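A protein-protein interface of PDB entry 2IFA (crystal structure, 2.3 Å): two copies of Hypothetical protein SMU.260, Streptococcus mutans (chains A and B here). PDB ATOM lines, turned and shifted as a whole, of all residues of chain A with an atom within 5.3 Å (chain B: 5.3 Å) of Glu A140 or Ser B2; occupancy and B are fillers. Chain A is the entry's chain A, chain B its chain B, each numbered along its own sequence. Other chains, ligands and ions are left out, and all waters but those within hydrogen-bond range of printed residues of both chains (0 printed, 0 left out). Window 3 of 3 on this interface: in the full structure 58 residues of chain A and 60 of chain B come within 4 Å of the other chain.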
ATOM      1  N   LEU A   7       6.229  14.314  24.337  1.00  0.00           N
ATOM      2  CA  LEU A   7       5.875  15.513  23.604  1.00  0.00           C
ATOM      3  C   LEU A   7       5.602  15.145  22.138  1.00  0.00           C
ATOM      4  O   LEU A   7       4.680  15.668  21.518  1.00  0.00           O
ATOM      5  CB  LEU A   7       7.011  16.531  23.695  1.00  0.00           C
ATOM      6  CG  LEU A   7       6.809  17.755  22.809  1.00  0.00           C
ATOM      7  CD1 LEU A   7       5.579  18.536  23.287  1.00  0.00           C
ATOM      8  CD2 LEU A   7       8.056  18.618  22.858  1.00  0.00           C
ATOM      9  N   GLN A  10       2.243  13.736  21.943  1.00  0.00           N
ATOM     10  CA  GLN A  10       1.238  14.758  22.203  1.00  0.00           C
ATOM     11  C   GLN A  10       0.907  15.565  20.947  1.00  0.00           C
ATOM     12  O   GLN A  10      -0.265  15.860  20.686  1.00  0.00           O
ATOM     13  CB  GLN A  10       1.717  15.699  23.302  1.00  0.00           C
ATOM     14  CG  GLN A  10       0.645  16.642  23.797  1.00  0.00           C
ATOM     15  CD  GLN A  10       1.110  17.495  24.963  1.00  0.00           C
ATOM     16  OE1 GLN A  10       1.819  17.020  25.842  1.00  0.00           O
ATOM     17  NE2 GLN A  10       0.695  18.753  24.982  1.00  0.00           N
ATOM     18  N   TRP A 135       5.881  23.252  15.591  1.00  0.00           N
ATOM     19  CA  TRP A 135       4.821  22.315  15.930  1.00  0.00           C
ATOM     20  C   TRP A 135       5.031  21.757  17.352  1.00  0.00           C
ATOM     21  O   TRP A 135       4.094  21.609  18.134  1.00  0.00           O
ATOM     22  CB  TRP A 135       4.819  21.166  14.919  1.00  0.00           C
ATOM     23  CG  TRP A 135       3.455  20.660  14.555  1.00  0.00           C
ATOM     24  CD1 TRP A 135       2.321  20.763  15.299  1.00  0.00           C
ATOM     25  CD2 TRP A 135       3.085  19.970  13.349  1.00  0.00           C
ATOM     26  NE1 TRP A 135       1.267  20.188  14.638  1.00  0.00           N
ATOM     27  CE2 TRP A 135       1.706  19.692  13.440  1.00  0.00           C
ATOM     28  CE3 TRP A 135       3.783  19.565  12.202  1.00  0.00           C
ATOM     29  CZ2 TRP A 135       1.007  19.024  12.427  1.00  0.00           C
ATOM     30  CZ3 TRP A 135       3.082  18.900  11.188  1.00  0.00           C
ATOM     31  CH2 TRP A 135       1.713  18.639  11.310  1.00  0.00           C
ATOM     32  N   LEU A 136       6.273  21.424  17.659  1.00  0.00           N
ATOM     33  CA  LEU A 136       6.604  20.868  18.956  1.00  0.00           C
ATOM     34  C   LEU A 136       6.484  21.963  20.016  1.00  0.00           C
ATOM     35  O   LEU A 136       5.848  21.763  21.055  1.00  0.00           O
ATOM     36  CB  LEU A 136       8.027  20.274  18.907  1.00  0.00           C
ATOM     37  CG  LEU A 136       8.234  18.747  18.845  1.00  0.00           C
ATOM     38  CD1 LEU A 136       7.066  18.041  18.206  1.00  0.00           C
ATOM     39  CD2 LEU A 136       9.514  18.449  18.071  1.00  0.00           C
ATOM     40  N   ALA A 137       7.074  23.124  19.746  1.00  0.00           N
ATOM     41  CA  ALA A 137       7.016  24.218  20.709  1.00  0.00           C
ATOM     42  C   ALA A 137       5.564  24.550  21.083  1.00  0.00           C
ATOM     43  O   ALA A 137       5.252  24.728  22.256  1.00  0.00           O
ATOM     44  CB  ALA A 137       7.728  25.457  20.160  1.00  0.00           C
ATOM     45  N   LEU A 138       4.674  24.632  20.100  1.00  0.00           N
ATOM     46  CA  LEU A 138       3.275  24.948  20.393  1.00  0.00           C
ATOM     47  C   LEU A 138       2.541  23.797  21.070  1.00  0.00           C
ATOM     48  O   LEU A 138       1.752  24.011  21.990  1.00  0.00           O
ATOM     49  CB  LEU A 138       2.551  25.370  19.115  1.00  0.00           C
ATOM     50  CG  LEU A 138       2.649  26.852  18.732  1.00  0.00           C
ATOM     51  CD1 LEU A 138       4.102  27.338  18.708  1.00  0.00           C
ATOM     52  CD2 LEU A 138       1.996  27.036  17.375  1.00  0.00           C
ATOM     53  N   ALA A 139       2.815  22.572  20.641  1.00  0.00           N
ATOM     54  CA  ALA A 139       2.153  21.430  21.243  1.00  0.00           C
ATOM     55  C   ALA A 139       2.404  21.383  22.747  1.00  0.00           C
ATOM     56  O   ALA A 139       1.505  21.086  23.528  1.00  0.00           O
ATOM     57  CB  ALA A 139       2.632  20.145  20.590  1.00  0.00           C
ATOM     58  N   GLU A 140       3.626  21.683  23.160  1.00  0.00           N
ATOM     59  CA  GLU A 140       3.947  21.645  24.579  1.00  0.00           C
ATOM     60  C   GLU A 140       3.065  22.603  25.378  1.00  0.00           C
ATOM     61  O   GLU A 140       2.743  22.340  26.531  1.00  0.00           O
ATOM     62  CB  GLU A 140       5.413  21.997  24.810  1.00  0.00           C
ATOM     63  CG  GLU A 140       5.840  21.910  26.258  1.00  0.00           C
ATOM     64  CD  GLU A 140       7.252  22.408  26.479  1.00  0.00           C
ATOM     65  OE1 GLU A 140       7.569  23.523  26.017  1.00  0.00           O
ATOM     66  OE2 GLU A 140       8.048  21.688  27.121  1.00  0.00           O
ATOM     67  N   GLN A 141       2.697  23.715  24.746  1.00  0.00           N
ATOM     68  CA  GLN A 141       1.855  24.748  25.352  1.00  0.00           C
ATOM     69  C   GLN A 141       0.377  24.478  25.091  1.00  0.00           C
ATOM     70  O   GLN A 141      -0.453  25.361  25.264  1.00  0.00           O
ATOM     71  CB  GLN A 141       2.206  26.116  24.763  1.00  0.00           C
ATOM     72  CG  GLN A 141       3.639  26.544  24.970  1.00  0.00           C
ATOM     73  CD  GLN A 141       3.951  26.754  26.424  1.00  0.00           C
ATOM     74  OE1 GLN A 141       3.381  27.635  27.072  1.00  0.00           O
ATOM     75  NE2 GLN A 141       4.850  25.942  26.956  1.00  0.00           N
ATOM     76  N   ASN A 142       0.062  23.261  24.660  1.00  0.00           N
ATOM     77  CA  ASN A 142      -1.317  22.885  24.363  1.00  0.00           C
ATOM     78  C   ASN A 142      -1.922  23.743  23.262  1.00  0.00           C
ATOM     79  O   ASN A 142      -3.133  23.966  23.238  1.00  0.00           O
ATOM     80  CB  ASN A 142      -2.193  22.992  25.614  1.00  0.00           C
ATOM     81  CG  ASN A 142      -1.746  22.066  26.709  1.00  0.00           C
ATOM     82  OD1 ASN A 142      -1.552  22.488  27.847  1.00  0.00           O
ATOM     83  ND2 ASN A 142      -1.583  20.791  26.379  1.00  0.00           N
ATOM     84  N   SER B   2      11.015  23.145  32.242  1.00  0.00           N
ATOM     85  CA  SER B   2      12.035  22.930  31.187  1.00  0.00           C
ATOM     86  C   SER B   2      11.278  22.654  29.898  1.00  0.00           C
ATOM     87  O   SER B   2      10.953  21.517  29.572  1.00  0.00           O
ATOM     88  CB  SER B   2      12.949  21.750  31.557  1.00  0.00           C
ATOM     89  OG  SER B   2      14.160  21.765  30.814  1.00  0.00           O
ATOM     90  N   ASN B   3      11.006  23.718  29.162  1.00  0.00           N
ATOM     91  CA  ASN B   3      10.268  23.610  27.925  1.00  0.00           C
ATOM     92  C   ASN B   3      11.072  22.974  26.798  1.00  0.00           C
ATOM     93  O   ASN B   3      12.177  22.441  26.987  1.00  0.00           O
ATOM     94  CB  ASN B   3       9.780  24.997  27.509  1.00  0.00           C
ATOM     95  CG  ASN B   3      10.834  26.054  27.708  1.00  0.00           C
ATOM     96  OD1 ASN B   3      12.028  25.794  27.515  1.00  0.00           O
ATOM     97  ND2 ASN B   3      10.404  27.264  28.088  1.00  0.00           N
ATOM     98  N   PHE B   4      10.481  23.039  25.616  1.00  0.00           N
ATOM     99  CA  PHE B   4      11.072  22.499  24.415  1.00  0.00           C
ATOM    100  C   PHE B   4      12.292  23.319  24.012  1.00  0.00           C
ATOM    101  O   PHE B   4      13.279  22.786  23.514  1.00  0.00           O
ATOM    102  CB  PHE B   4      10.033  22.527  23.311  1.00  0.00           C
ATOM    103  CG  PHE B   4      10.521  21.994  22.021  1.00  0.00           C
ATOM    104  CD1 PHE B   4      11.071  20.724  21.958  1.00  0.00           C
ATOM    105  CD2 PHE B   4      10.424  22.755  20.866  1.00  0.00           C
ATOM    106  CE1 PHE B   4      11.528  20.216  20.753  1.00  0.00           C
ATOM    107  CE2 PHE B   4      10.872  22.258  19.662  1.00  0.00           C
ATOM    108  CZ  PHE B   4      11.428  20.984  19.602  1.00  0.00           C
ATOM    109  N   LEU B   5      12.224  24.622  24.237  1.00  0.00           N
ATOM    110  CA  LEU B   5      13.331  25.497  23.890  1.00  0.00           C
ATOM    111  C   LEU B   5      14.641  25.112  24.564  1.00  0.00           C
ATOM    112  O   LEU B   5      15.705  25.329  23.985  1.00  0.00           O
ATOM    113  CB  LEU B   5      13.001  26.951  24.236  1.00  0.00           C
ATOM    114  CG  LEU B   5      12.706  27.869  23.047  1.00  0.00           C
ATOM    115  CD1 LEU B   5      13.922  27.973  22.112  1.00  0.00           C
ATOM    116  CD2 LEU B   5      11.481  27.307  22.314  1.00  0.00           C
ATOM    117  N   ASP B   6      14.579  24.558  25.778  1.00  0.00           N
ATOM    118  CA  ASP B   6      15.800  24.169  26.490  1.00  0.00           C
ATOM    119  C   ASP B   6      16.482  23.063  25.686  1.00  0.00           C
ATOM    120  O   ASP B   6      17.671  23.142  25.371  1.00  0.00           O
ATOM    121  CB  ASP B   6      15.497  23.630  27.903  1.00  0.00           C
ATOM    122  CG  ASP B   6      14.917  24.686  28.857  1.00  0.00           C
ATOM    123  OD1 ASP B   6      15.336  25.862  28.830  1.00  0.00           O
ATOM    124  OD2 ASP B   6      14.046  24.317  29.676  1.00  0.00           O
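The backbone NH (N) of Phe B4 sits at hydrogen-bond distance from the side-chain carboxylate (OE1) of Glu A140.
The side-chain hydroxyl of Ser B2 is in hydrogen-bond range of the side-chain carboxylate of Asp B6, 2.8 Å away. The side-chain amide oxygen (OD1) of Asn B3 lies close to the backbone NH (N) of Leu B5 (3.5 Å). N of Asn B3 is in hydrogen-bond range of OD2 of Asp B6 (3.1 Å).
Phe B4 touches Leu A7. CD2 of Leu A136 touches CZ of Phe B4 (3.5 Å). Ala A137 touches Phe B4 (N to CD2, 3.6 Å). Glu A140 touches Ser B2. Asn B3 touches Glu A140.
Of the printed residues of chain B, Leu A7 touches Phe B4 (3.8 Å). Of the printed residues of chain B, Ala A137 touches Phe B4. Glu A140 touches just these residues of chain B: Ser B2, Asn B3 and Phe B4. Of the printed residues of chain A, Ser B2 touches Glu A140. Printed residues of chain A within 4 Å of Asn B3: Glu A140 (3.0 Å). Of the printed residues of chain A, Phe B4 touches Leu A7 (3.8 Å), Leu A136 (3.5 Å), Ala A137 (3.6 Å) and Glu A140 (3.0 Å). Leu B5 touches none of the printed residues of chain A. The nearest residue of chain B that does not touch Glu A140 is Leu B5 (5.1 Å).
Of the 10 printed residues of chain A, 4 touch a printed residue of chain B. Hydrophobic or aromatic side chains of chain A within 4 Å of the printed part of chain B: Leu A7, Leu A136 and Ala A137. Of the 5 printed residues of chain B, 3 touch a printed residue of chain A. Printed residues of chain B that touch a printed residue of chain A: Ser B2, Asn B3 and Phe B4. Among the printed residues, 6 pairs touch across the chains. Among the printed residues, no Asp or Glu carboxylate lies within 4 Å of a Lys or Arg side-chain nitrogen of the other chain.
No position is printed for both chains.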
